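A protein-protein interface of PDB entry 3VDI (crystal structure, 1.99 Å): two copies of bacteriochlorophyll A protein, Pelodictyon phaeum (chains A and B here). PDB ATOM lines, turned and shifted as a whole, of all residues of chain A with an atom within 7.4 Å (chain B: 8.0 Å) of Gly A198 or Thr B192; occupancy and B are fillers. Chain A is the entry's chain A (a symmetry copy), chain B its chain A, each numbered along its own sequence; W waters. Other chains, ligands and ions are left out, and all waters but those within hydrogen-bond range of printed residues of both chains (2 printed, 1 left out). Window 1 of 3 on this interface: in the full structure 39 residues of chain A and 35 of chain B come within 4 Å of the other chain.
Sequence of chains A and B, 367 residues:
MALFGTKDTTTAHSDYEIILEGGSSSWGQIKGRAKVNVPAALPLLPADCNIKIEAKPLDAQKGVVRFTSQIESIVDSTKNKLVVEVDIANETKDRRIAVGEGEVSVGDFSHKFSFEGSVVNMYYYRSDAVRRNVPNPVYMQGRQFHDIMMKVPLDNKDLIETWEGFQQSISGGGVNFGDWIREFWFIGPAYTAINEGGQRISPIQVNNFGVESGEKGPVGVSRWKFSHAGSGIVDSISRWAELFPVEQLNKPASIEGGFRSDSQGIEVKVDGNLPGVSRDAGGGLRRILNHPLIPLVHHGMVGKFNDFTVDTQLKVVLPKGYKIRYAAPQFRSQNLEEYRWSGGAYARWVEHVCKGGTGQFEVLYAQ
OG of Ser A231 is in hydrogen-bond range of O of Gly B188, at 2.6 Å.
O of Asn A195 is in hydrogen-bond range of OG1 of Thr B192 (3.3 Å).
O of Glu A196 lies within hydrogen-bond range of OG1 of Thr B192.
N of Gly A198 lies within hydrogen-bond range of OG1 of Thr B192 (3.3 Å).
NH1 of Arg A200 lies within salt-bridge range of OE2 of Glu B183, 2.8 Å away.
O of Gly A198 sits at hydrogen-bond distance from N of Ser A231.
The backbone carbonyl oxygen (O) of Phe B186 lies within hydrogen-bond range of the backbone NH (N) of Tyr B191.
The backbone NH (N) of Arg A200 lies within hydrogen-bond range of the backbone carbonyl oxygen (O) of Ala A229 (3.0 Å).
Tyr B191 touches Asn A195.
Asn A195 touches Asn B195.
Gly A198 touches Tyr B191.
CD of Arg A200 touches OH of Tyr B191, at 3.3 Å.
Glu B183 touches Ala A229 (OE1 to CB, 3.4 Å).
CA of Ser A231 touches O of Glu B183, at 3.2 Å.
O of Phe B186 touches CB of Ser A231 (3.3 Å).
Ser A231 touches Ile B187.
Ser A231 touches Tyr B191.
Gly B188 touches Ile A233.
Of the printed residues of chain B, Asn A195 touches Tyr B191 (3.9 Å), Thr B192 (3.3 Å) and Asn B195 (3.8 Å).
No residue of chain B comes within 4 Å of Gly A197.
Gly A198 touches just these residues of chain B: Tyr B191 (3.8 Å) and Thr B192 (3.3 Å).
Printed residues of chain B within 4 Å of Ala A229: Glu B183 (3.4 Å).
Printed residues of chain A within 4 Å of Phe B186: Ser A231 (3.3 Å).
Of the printed residues of chain A, Ile B187 touches Ser A231 (3.6 Å).
Of the printed residues of chain A, Gly B188 touches Ser A231 and Ile A233.
Ala B190 touches none of the printed residues of chain A.
Thr B192 touches just these residues of chain A: Asn A195 (3.3 Å), Glu A196 (3.3 Å) and Gly A198 (3.3 Å).
His B298 touches none of the printed residues of chain A.
The nearest printed residue of chain A that does not touch Gly B188 is Gly A232 (4.4 Å).
Hydrophobic or aromatic side chains of chain A that line the printed part of chain B: Ala A229 and Ile A233.
Along chain A the printed residues that touch a printed residue of chain B span positions 195 to 233.
Among the printed residues, 16 pairs touch across the chains.
Among the printed residues, Asp or Glu carboxylates within 4 Å of a Lys or Arg side-chain nitrogen of the other chain: Arg A200 with Glu B183 (2.8 Å).
Asn A195 touches its own counterpart, Asn B195.
Of the 16 pairs that touch across the chains among the printed residues, 1 has its exchanged pair printed and touching as well.
Water W1 bridges the backbone carbonyl oxygen of Glu A196 (2.6 Å) and the side-chain hydroxyl of Thr B192 (3.1 Å).
Water W2 lies within hydrogen-bond range of the side-chain carboxylate (OE1) of Glu B196 (2.9 Å) and the side-chain carboxylate (OE1) of Glu A196 (3.0 Å).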
ATOM      1  N   GLY A 142     -17.200 -11.620 -21.687  1.00  0.00           N
ATOM      2  CA  GLY A 142     -16.897 -10.350 -22.356  1.00  0.00           C
ATOM      3  C   GLY A 142     -17.957  -9.913 -23.327  1.00  0.00           C
ATOM      4  O   GLY A 142     -18.982 -10.578 -23.467  1.00  0.00           O
ATOM      5  N   ALA A 193     -30.388 -20.771 -30.682  1.00  0.00           N
ATOM      6  CA  ALA A 193     -28.985 -21.082 -30.393  1.00  0.00           C
ATOM      7  C   ALA A 193     -28.248 -19.952 -29.639  1.00  0.00           C
ATOM      8  O   ALA A 193     -27.249 -20.232 -28.982  1.00  0.00           O
ATOM      9  CB  ALA A 193     -28.247 -21.435 -31.677  1.00  0.00           C
ATOM     10  N   ILE A 194     -28.737 -18.698 -29.732  1.00  0.00           N
ATOM     11  CA  ILE A 194     -28.106 -17.541 -29.054  1.00  0.00           C
ATOM     12  C   ILE A 194     -28.001 -17.828 -27.555  1.00  0.00           C
ATOM     13  O   ILE A 194     -26.886 -17.977 -27.038  1.00  0.00           O
ATOM     14  CB  ILE A 194     -28.799 -16.173 -29.359  1.00  0.00           C
ATOM     15  CG1 ILE A 194     -28.735 -15.831 -30.878  1.00  0.00           C
ATOM     16  CG2 ILE A 194     -28.179 -15.028 -28.490  1.00  0.00           C
ATOM     17  CD1 ILE A 194     -29.707 -14.735 -31.348  1.00  0.00           C
ATOM     18  N   ASN A 195     -29.150 -18.034 -26.899  1.00  0.00           N
ATOM     19  CA  ASN A 195     -29.205 -18.343 -25.458  1.00  0.00           C
ATOM     20  C   ASN A 195     -28.487 -19.616 -25.076  1.00  0.00           C
ATOM     21  O   ASN A 195     -27.924 -19.701 -23.986  1.00  0.00           O
ATOM     22  CB  ASN A 195     -30.650 -18.390 -24.965  1.00  0.00           C
ATOM     23  CG  ASN A 195     -30.759 -18.572 -23.472  1.00  0.00           C
ATOM     24  OD1 ASN A 195     -30.550 -17.650 -22.693  1.00  0.00           O
ATOM     25  ND2 ASN A 195     -31.045 -19.780 -23.047  1.00  0.00           N
ATOM     26  N   GLU A 196     -28.536 -20.617 -25.961  1.00  0.00           N
ATOM     27  CA  GLU A 196     -27.916 -21.918 -25.774  1.00  0.00           C
ATOM     28  C   GLU A 196     -26.414 -21.824 -25.456  1.00  0.00           C
ATOM     29  O   GLU A 196     -25.924 -22.583 -24.628  1.00  0.00           O
ATOM     30  CB  GLU A 196     -28.191 -22.802 -27.002  1.00  0.00           C
ATOM     31  CG  GLU A 196     -27.875 -24.266 -26.766  1.00  0.00           C
ATOM     32  CD  GLU A 196     -28.812 -24.998 -25.821  1.00  0.00           C
ATOM     33  OE1 GLU A 196     -29.888 -24.450 -25.488  1.00  0.00           O
ATOM     34  OE2 GLU A 196     -28.457 -26.121 -25.399  1.00  0.00           O
ATOM     35  N   GLY A 197     -25.708 -20.910 -26.112  1.00  0.00           N
ATOM     36  CA  GLY A 197     -24.283 -20.723 -25.857  1.00  0.00           C
ATOM     37  C   GLY A 197     -23.970 -19.651 -24.829  1.00  0.00           C
ATOM     38  O   GLY A 197     -22.855 -19.143 -24.822  1.00  0.00           O
ATOM     39  N   GLY A 198     -24.947 -19.258 -23.999  1.00  0.00           N
ATOM     40  CA  GLY A 198     -24.745 -18.167 -23.019  1.00  0.00           C
ATOM     41  C   GLY A 198     -24.378 -16.873 -23.722  1.00  0.00           C
ATOM     42  O   GLY A 198     -23.569 -16.073 -23.236  1.00  0.00           O
ATOM     43  N   GLN A 199     -24.949 -16.687 -24.919  1.00  0.00           N
ATOM     44  CA  GLN A 199     -24.636 -15.567 -25.781  1.00  0.00           C
ATOM     45  C   GLN A 199     -25.762 -14.568 -25.780  1.00  0.00           C
ATOM     46  O   GLN A 199     -26.896 -14.919 -25.478  1.00  0.00           O
ATOM     47  CB  GLN A 199     -24.340 -16.071 -27.203  1.00  0.00           C
ATOM     48  CG  GLN A 199     -23.694 -15.040 -28.157  1.00  0.00           C
ATOM     49  CD  GLN A 199     -23.141 -15.735 -29.379  1.00  0.00           C
ATOM     50  OE1 GLN A 199     -23.315 -16.947 -29.577  1.00  0.00           O
ATOM     51  NE2 GLN A 199     -22.373 -15.010 -30.169  1.00  0.00           N
ATOM     52  N   ARG A 200     -25.427 -13.294 -26.054  1.00  0.00           N
ATOM     53  CA  ARG A 200     -26.418 -12.218 -26.155  1.00  0.00           C
ATOM     54  C   ARG A 200     -26.162 -11.422 -27.438  1.00  0.00           C
ATOM     55  O   ARG A 200     -25.011 -11.202 -27.787  1.00  0.00           O
ATOM     56  CB  ARG A 200     -26.278 -11.268 -24.951  1.00  0.00           C
ATOM     57  CG  ARG A 200     -26.629 -11.904 -23.613  1.00  0.00           C
ATOM     58  CD  ARG A 200     -26.584 -10.890 -22.486  1.00  0.00           C
ATOM     59  NE  ARG A 200     -27.702  -9.934 -22.553  1.00  0.00           N
ATOM     60  CZ  ARG A 200     -27.805  -8.840 -21.803  1.00  0.00           C
ATOM     61  NH1 ARG A 200     -26.835  -8.513 -20.954  1.00  0.00           N
ATOM     62  NH2 ARG A 200     -28.843  -8.030 -21.941  1.00  0.00           N
ATOM     63  N   ALA A 229     -22.293 -10.596 -26.632  1.00  0.00           N
ATOM     64  CA  ALA A 229     -21.601 -10.870 -25.379  1.00  0.00           C
ATOM     65  C   ALA A 229     -21.667 -12.352 -25.080  1.00  0.00           C
ATOM     66  O   ALA A 229     -22.471 -13.065 -25.669  1.00  0.00           O
ATOM     67  CB  ALA A 229     -22.235 -10.076 -24.241  1.00  0.00           C
ATOM     68  N   GLY A 230     -20.799 -12.796 -24.190  1.00  0.00           N
ATOM     69  CA  GLY A 230     -20.742 -14.190 -23.772  1.00  0.00           C
ATOM     70  C   GLY A 230     -20.366 -14.336 -22.313  1.00  0.00           C
ATOM     71  O   GLY A 230     -19.641 -13.502 -21.763  1.00  0.00           O
ATOM     72  N   SER A 231     -20.909 -15.354 -21.671  1.00  0.00           N
ATOM     73  CA  SER A 231     -20.618 -15.712 -20.270  1.00  0.00           C
ATOM     74  C   SER A 231     -19.352 -16.602 -20.189  1.00  0.00           C
ATOM     75  O   SER A 231     -18.930 -16.989 -19.092  1.00  0.00           O
ATOM     76  CB  SER A 231     -21.804 -16.447 -19.651  1.00  0.00           C
ATOM     77  OG  SER A 231     -22.015 -17.656 -20.363  1.00  0.00           O
ATOM     78  N   GLY A 232     -18.749 -16.898 -21.338  1.00  0.00           N
ATOM     79  CA  GLY A 232     -17.500 -17.673 -21.394  1.00  0.00           C
ATOM     80  C   GLY A 232     -17.459 -18.812 -22.386  1.00  0.00           C
ATOM     81  O   GLY A 232     -16.372 -19.312 -22.710  1.00  0.00           O
ATOM     82  N   ILE A 233     -18.639 -19.274 -22.845  1.00  0.00           N
ATOM     83  CA  ILE A 233     -18.744 -20.377 -23.829  1.00  0.00           C
ATOM     84  C   ILE A 233     -18.400 -19.815 -25.218  1.00  0.00           C
ATOM     85  O   ILE A 233     -17.831 -20.528 -26.040  1.00  0.00           O
ATOM     86  CB  ILE A 233     -20.178 -21.000 -23.794  1.00  0.00           C
ATOM     87  CG1 ILE A 233     -20.490 -21.644 -22.409  1.00  0.00           C
ATOM     88  CG2 ILE A 233     -20.421 -22.012 -24.937  1.00  0.00           C
ATOM     89  CD1 ILE A 233     -22.014 -21.759 -22.094  1.00  0.00           C
ATOM     90  N   VAL A 234     -18.753 -18.513 -25.459  1.00  0.00           N
ATOM     91  CA  VAL A 234     -18.541 -17.831 -26.730  1.00  0.00           C
ATOM     92  C   VAL A 234     -17.024 -17.655 -26.980  1.00  0.00           C
ATOM     93  O   VAL A 234     -16.367 -16.787 -26.376  1.00  0.00           O
ATOM     94  CB  VAL A 234     -19.364 -16.506 -26.848  1.00  0.00           C
ATOM     95  CG1 VAL A 234     -19.204 -15.867 -28.224  1.00  0.00           C
ATOM     96  CG2 VAL A 234     -20.842 -16.749 -26.555  1.00  0.00           C
ATOM     97  N   ILE A 237     -15.231 -14.481 -28.293  1.00  0.00           N
ATOM     98  CA  ILE A 237     -14.905 -13.504 -27.268  1.00  0.00           C
ATOM     99  C   ILE A 237     -13.823 -14.039 -26.333  1.00  0.00           C
ATOM    100  O   ILE A 237     -12.816 -13.354 -26.091  1.00  0.00           O
ATOM    101  CB  ILE A 237     -16.180 -13.092 -26.508  1.00  0.00           C
ATOM    102  CG1 ILE A 237     -17.151 -12.319 -27.444  1.00  0.00           C
ATOM    103  CG2 ILE A 237     -15.811 -12.271 -25.241  1.00  0.00           C
ATOM    104  CD1 ILE A 237     -18.578 -12.253 -26.925  1.00  0.00           C
ATOM    105  N   ILE A 294     -18.624 -23.439 -28.458  1.00  0.00           N
ATOM    106  CA  ILE A 294     -19.787 -23.126 -29.302  1.00  0.00           C
ATOM    107  C   ILE A 294     -20.119 -24.250 -30.285  1.00  0.00           C
ATOM    108  O   ILE A 294     -21.267 -24.689 -30.270  1.00  0.00           O
ATOM    109  CB  ILE A 294     -19.647 -21.729 -29.989  1.00  0.00           C
ATOM    110  CG1 ILE A 294     -19.850 -20.562 -28.977  1.00  0.00           C
ATOM    111  CG2 ILE A 294     -20.524 -21.610 -31.290  1.00  0.00           C
ATOM    112  CD1 ILE A 294     -21.373 -20.321 -28.377  1.00  0.00           C
ATOM    113  N   VAL A 297     -21.811 -27.008 -28.211  1.00  0.00           N
ATOM    114  CA  VAL A 297     -23.076 -26.543 -27.657  1.00  0.00           C
ATOM    115  C   VAL A 297     -24.160 -26.400 -28.730  1.00  0.00           C
ATOM    116  O   VAL A 297     -25.279 -26.879 -28.533  1.00  0.00           O
ATOM    117  CB  VAL A 297     -22.891 -25.295 -26.768  1.00  0.00           C
ATOM    118  CG1 VAL A 297     -24.231 -24.773 -26.308  1.00  0.00           C
ATOM    119  CG2 VAL A 297     -22.000 -25.626 -25.558  1.00  0.00           C
ATOM    120  N   HIS A 298     -23.798 -25.828 -29.891  1.00  0.00           N
ATOM    121  CA  HIS A 298     -24.726 -25.676 -31.006  1.00  0.00           C
ATOM    122  C   HIS A 298     -25.072 -27.011 -31.655  1.00  0.00           C
ATOM    123  O   HIS A 298     -26.244 -27.272 -31.898  1.00  0.00           O
ATOM    124  CB  HIS A 298     -24.186 -24.668 -32.017  1.00  0.00           C
ATOM    125  CG  HIS A 298     -24.226 -23.247 -31.530  1.00  0.00           C
ATOM    126  ND1 HIS A 298     -23.896 -22.197 -32.361  1.00  0.00           N
ATOM    127  CD2 HIS A 298     -24.573 -22.749 -30.313  1.00  0.00           C
ATOM    128  CE1 HIS A 298     -24.048 -21.100 -31.632  1.00  0.00           C
ATOM    129  NE2 HIS A 298     -24.477 -21.384 -30.401  1.00  0.00           N
ATOM    130  N   GLU B 183     -24.003 -11.480 -17.578  1.00  0.00           N
ATOM    131  CA  GLU B 183     -23.211 -12.521 -18.253  1.00  0.00           C
ATOM    132  C   GLU B 183     -21.846 -12.723 -17.597  1.00  0.00           C
ATOM    133  O   GLU B 183     -21.210 -13.714 -17.849  1.00  0.00           O
ATOM    134  CB  GLU B 183     -23.099 -12.304 -19.776  1.00  0.00           C
ATOM    135  CG  GLU B 183     -22.542 -10.945 -20.192  1.00  0.00           C
ATOM    136  CD  GLU B 183     -23.560  -9.861 -20.492  1.00  0.00           C
ATOM    137  OE1 GLU B 183     -23.205  -8.903 -21.211  1.00  0.00           O
ATOM    138  OE2 GLU B 183     -24.684  -9.920 -19.945  1.00  0.00           O
ATOM    139  N   PHE B 186     -23.284 -14.864 -14.228  1.00  0.00           N
ATOM    140  CA  PHE B 186     -23.710 -16.214 -14.547  1.00  0.00           C
ATOM    141  C   PHE B 186     -22.754 -16.866 -15.537  1.00  0.00           C
ATOM    142  O   PHE B 186     -23.069 -17.105 -16.710  1.00  0.00           O
ATOM    143  CB  PHE B 186     -25.212 -16.241 -14.904  1.00  0.00           C
ATOM    144  CG  PHE B 186     -26.033 -15.854 -13.687  1.00  0.00           C
ATOM    145  CD1 PHE B 186     -26.153 -16.720 -12.600  1.00  0.00           C
ATOM    146  CD2 PHE B 186     -26.608 -14.580 -13.585  1.00  0.00           C
ATOM    147  CE1 PHE B 186     -26.874 -16.338 -11.451  1.00  0.00           C
ATOM    148  CE2 PHE B 186     -27.335 -14.207 -12.441  1.00  0.00           C
ATOM    149  CZ  PHE B 186     -27.453 -15.088 -11.387  1.00  0.00           C
ATOM    150  N   ILE B 187     -21.527 -17.114 -15.037  1.00  0.00           N
ATOM    151  CA  ILE B 187     -20.393 -17.640 -15.810  1.00  0.00           C
ATOM    152  C   ILE B 187     -20.736 -18.911 -16.585  1.00  0.00           C
ATOM    153  O   ILE B 187     -21.489 -19.754 -16.088  1.00  0.00           O
ATOM    154  CB  ILE B 187     -19.112 -17.777 -14.918  1.00  0.00           C
ATOM    155  CG1 ILE B 187     -17.818 -18.013 -15.773  1.00  0.00           C
ATOM    156  CG2 ILE B 187     -19.286 -18.836 -13.782  1.00  0.00           C
ATOM    157  CD1 ILE B 187     -16.491 -17.953 -14.987  1.00  0.00           C
ATOM    158  N   GLY B 188     -20.231 -19.010 -17.808  1.00  0.00           N
ATOM    159  CA  GLY B 188     -20.445 -20.190 -18.648  1.00  0.00           C
ATOM    160  C   GLY B 188     -21.910 -20.586 -18.790  1.00  0.00           C
ATOM    161  O   GLY B 188     -22.763 -19.733 -19.056  1.00  0.00           O
ATOM    162  N   PRO B 189     -22.244 -21.882 -18.621  1.00  0.00           N
ATOM    163  CA  PRO B 189     -23.635 -22.302 -18.800  1.00  0.00           C
ATOM    164  C   PRO B 189     -24.561 -21.948 -17.648  1.00  0.00           C
ATOM    165  O   PRO B 189     -25.741 -22.294 -17.728  1.00  0.00           O
ATOM    166  CB  PRO B 189     -23.513 -23.807 -19.031  1.00  0.00           C
ATOM    167  CG  PRO B 189     -22.354 -24.188 -18.136  1.00  0.00           C
ATOM    168  CD  PRO B 189     -21.379 -23.039 -18.290  1.00  0.00           C
ATOM    169  N   ALA B 190     -24.066 -21.237 -16.600  1.00  0.00           N
ATOM    170  CA  ALA B 190     -24.978 -20.755 -15.545  1.00  0.00           C
ATOM    171  C   ALA B 190     -25.945 -19.755 -16.198  1.00  0.00           C
ATOM    172  O   ALA B 190     -27.120 -19.710 -15.827  1.00  0.00           O
ATOM    173  CB  ALA B 190     -24.216 -20.081 -14.410  1.00  0.00           C
ATOM    174  N   TYR B 191     -25.464 -18.996 -17.199  1.00  0.00           N
ATOM    175  CA  TYR B 191     -26.313 -18.028 -17.920  1.00  0.00           C
ATOM    176  C   TYR B 191     -27.458 -18.756 -18.653  1.00  0.00           C
ATOM    177  O   TYR B 191     -28.616 -18.365 -18.528  1.00  0.00           O
ATOM    178  CB  TYR B 191     -25.499 -17.174 -18.916  1.00  0.00           C
ATOM    179  CG  TYR B 191     -26.324 -16.067 -19.540  1.00  0.00           C
ATOM    180  CD1 TYR B 191     -26.376 -14.798 -18.963  1.00  0.00           C
ATOM    181  CD2 TYR B 191     -27.098 -16.301 -20.677  1.00  0.00           C
ATOM    182  CE1 TYR B 191     -27.156 -13.781 -19.521  1.00  0.00           C
ATOM    183  CE2 TYR B 191     -27.863 -15.285 -21.254  1.00  0.00           C
ATOM    184  CZ  TYR B 191     -27.889 -14.029 -20.672  1.00  0.00           C
ATOM    185  OH  TYR B 191     -28.678 -13.047 -21.221  1.00  0.00           O
ATOM    186  N   THR B 192     -27.119 -19.805 -19.405  1.00  0.00           N
ATOM    187  CA  THR B 192     -28.064 -20.636 -20.167  1.00  0.00           C
ATOM    188  C   THR B 192     -29.142 -21.238 -19.273  1.00  0.00           C
ATOM    189  O   THR B 192     -30.300 -21.330 -19.687  1.00  0.00           O
ATOM    190  CB  THR B 192     -27.284 -21.768 -20.918  1.00  0.00           C
ATOM    191  OG1 THR B 192     -26.176 -21.195 -21.618  1.00  0.00           O
ATOM    192  CG2 THR B 192     -28.146 -22.509 -21.905  1.00  0.00           C
ATOM    193  N   ALA B 193     -28.744 -21.677 -18.064  1.00  0.00           N
ATOM    194  CA  ALA B 193     -29.635 -22.326 -17.099  1.00  0.00           C
ATOM    195  C   ALA B 193     -30.761 -21.401 -16.585  1.00  0.00           C
ATOM    196  O   ALA B 193     -31.783 -21.909 -16.131  1.00  0.00           O
ATOM    197  CB  ALA B 193     -28.832 -22.885 -15.933  1.00  0.00           C
ATOM    198  N   ILE B 194     -30.576 -20.067 -16.660  1.00  0.00           N
ATOM    199  CA  ILE B 194     -31.588 -19.091 -16.191  1.00  0.00           C
ATOM    200  C   ILE B 194     -32.916 -19.358 -16.901  1.00  0.00           C
ATOM    201  O   ILE B 194     -33.885 -19.772 -16.252  1.00  0.00           O
ATOM    202  CB  ILE B 194     -31.131 -17.600 -16.307  1.00  0.00           C
ATOM    203  CG1 ILE B 194     -29.872 -17.323 -15.431  1.00  0.00           C
ATOM    204  CG2 ILE B 194     -32.303 -16.628 -15.944  1.00  0.00           C
ATOM    205  CD1 ILE B 194     -29.111 -16.028 -15.763  1.00  0.00           C
ATOM    206  N   ASN B 195     -32.917 -19.250 -18.237  1.00  0.00           N
ATOM    207  CA  ASN B 195     -34.116 -19.499 -19.058  1.00  0.00           C
ATOM    208  C   ASN B 195     -34.661 -20.903 -18.937  1.00  0.00           C
ATOM    209  O   ASN B 195     -35.872 -21.101 -19.017  1.00  0.00           O
ATOM    210  CB  ASN B 195     -33.850 -19.168 -20.526  1.00  0.00           C
ATOM    211  CG  ASN B 195     -35.081 -19.279 -21.390  1.00  0.00           C
ATOM    212  OD1 ASN B 195     -35.955 -18.421 -21.380  1.00  0.00           O
ATOM    213  ND2 ASN B 195     -35.190 -20.365 -22.118  1.00  0.00           N
ATOM    214  N   GLU B 196     -33.762 -21.880 -18.779  1.00  0.00           N
ATOM    215  CA  GLU B 196     -34.088 -23.291 -18.652  1.00  0.00           C
ATOM    216  C   GLU B 196     -35.094 -23.573 -17.523  1.00  0.00           C
ATOM    217  O   GLU B 196     -35.972 -24.411 -17.691  1.00  0.00           O
ATOM    218  CB  GLU B 196     -32.795 -24.107 -18.489  1.00  0.00           C
ATOM    219  CG  GLU B 196     -33.001 -25.597 -18.679  1.00  0.00           C
ATOM    220  CD  GLU B 196     -33.302 -26.045 -20.099  1.00  0.00           C
ATOM    221  OE1 GLU B 196     -33.134 -25.234 -21.038  1.00  0.00           O
ATOM    222  OE2 GLU B 196     -33.723 -27.210 -20.267  1.00  0.00           O
ATOM    223  N   GLY B 197     -34.954 -22.883 -16.396  1.00  0.00           N
ATOM    224  CA  GLY B 197     -35.877 -23.058 -15.278  1.00  0.00           C
ATOM    225  C   GLY B 197     -37.033 -22.074 -15.269  1.00  0.00           C
ATOM    226  O   GLY B 197     -37.625 -21.865 -14.216  1.00  0.00           O
ATOM    227  N   GLY B 198     -37.330 -21.427 -16.404  1.00  0.00           N
ATOM    228  CA  GLY B 198     -38.395 -20.398 -16.459  1.00  0.00           C
ATOM    229  C   GLY B 198     -38.090 -19.257 -15.507  1.00  0.00           C
ATOM    230  O   GLY B 198     -38.983 -18.676 -14.878  1.00  0.00           O
ATOM    231  N   GLN B 199     -36.792 -18.962 -15.358  1.00  0.00           N
ATOM    232  CA  GLN B 199     -36.306 -17.979 -14.414  1.00  0.00           C
ATOM    233  C   GLN B 199     -35.870 -16.728 -15.128  1.00  0.00           C
ATOM    234  O   GLN B 199     -35.555 -16.773 -16.311  1.00  0.00           O
ATOM    235  CB  GLN B 199     -35.156 -18.577 -13.587  1.00  0.00           C
ATOM    236  CG  GLN B 199     -34.739 -17.767 -12.338  1.00  0.00           C
ATOM    237  CD  GLN B 199     -33.866 -18.609 -11.437  1.00  0.00           C
ATOM    238  OE1 GLN B 199     -33.485 -19.742 -11.769  1.00  0.00           O
ATOM    239  NE2 GLN B 199     -33.619 -18.121 -10.237  1.00  0.00           N
ATOM    240  N   HIS B 298     -32.066 -28.216 -14.086  1.00  0.00           N
ATOM    241  CA  HIS B 298     -30.664 -27.862 -14.287  1.00  0.00           C
ATOM    242  C   HIS B 298     -29.796 -29.082 -14.571  1.00  0.00           C
ATOM    243  O   HIS B 298     -28.996 -29.043 -15.498  1.00  0.00           O
ATOM    244  CB  HIS B 298     -30.145 -27.048 -13.104  1.00  0.00           C
ATOM    245  CG  HIS B 298     -30.698 -25.652 -13.045  1.00  0.00           C
ATOM    246  ND1 HIS B 298     -30.239 -24.740 -12.117  1.00  0.00           N
ATOM    247  CD2 HIS B 298     -31.643 -25.053 -13.815  1.00  0.00           C
ATOM    248  CE1 HIS B 298     -30.915 -23.623 -12.346  1.00  0.00           C
ATOM    249  NE2 HIS B 298     -31.753 -23.759 -13.374  1.00  0.00           N
ATOM    250  N   MET B 301     -29.712 -30.422 -18.095  1.00  0.00           N
ATOM    251  CA  MET B 301     -28.832 -29.811 -19.102  1.00  0.00           C
ATOM    252  C   MET B 301     -27.562 -30.633 -19.287  1.00  0.00           C
ATOM    253  O   MET B 301     -26.887 -30.492 -20.301  1.00  0.00           O
ATOM    254  CB  MET B 301     -28.514 -28.351 -18.755  1.00  0.00           C
ATOM    255  CG  MET B 301     -29.778 -27.508 -18.579  1.00  0.00           C
ATOM    256  SD  MET B 301     -29.430 -25.850 -17.960  1.00  0.00           S
ATOM    257  CE  MET B 301     -28.675 -25.139 -19.402  1.00  0.00           C
HETATM  258  O   HOH W   1     -24.710 -23.785 -22.639  1.00  0.00           O
HETATM  259  O   HOH W   2     -30.852 -25.105 -22.774  1.00  0.00           O
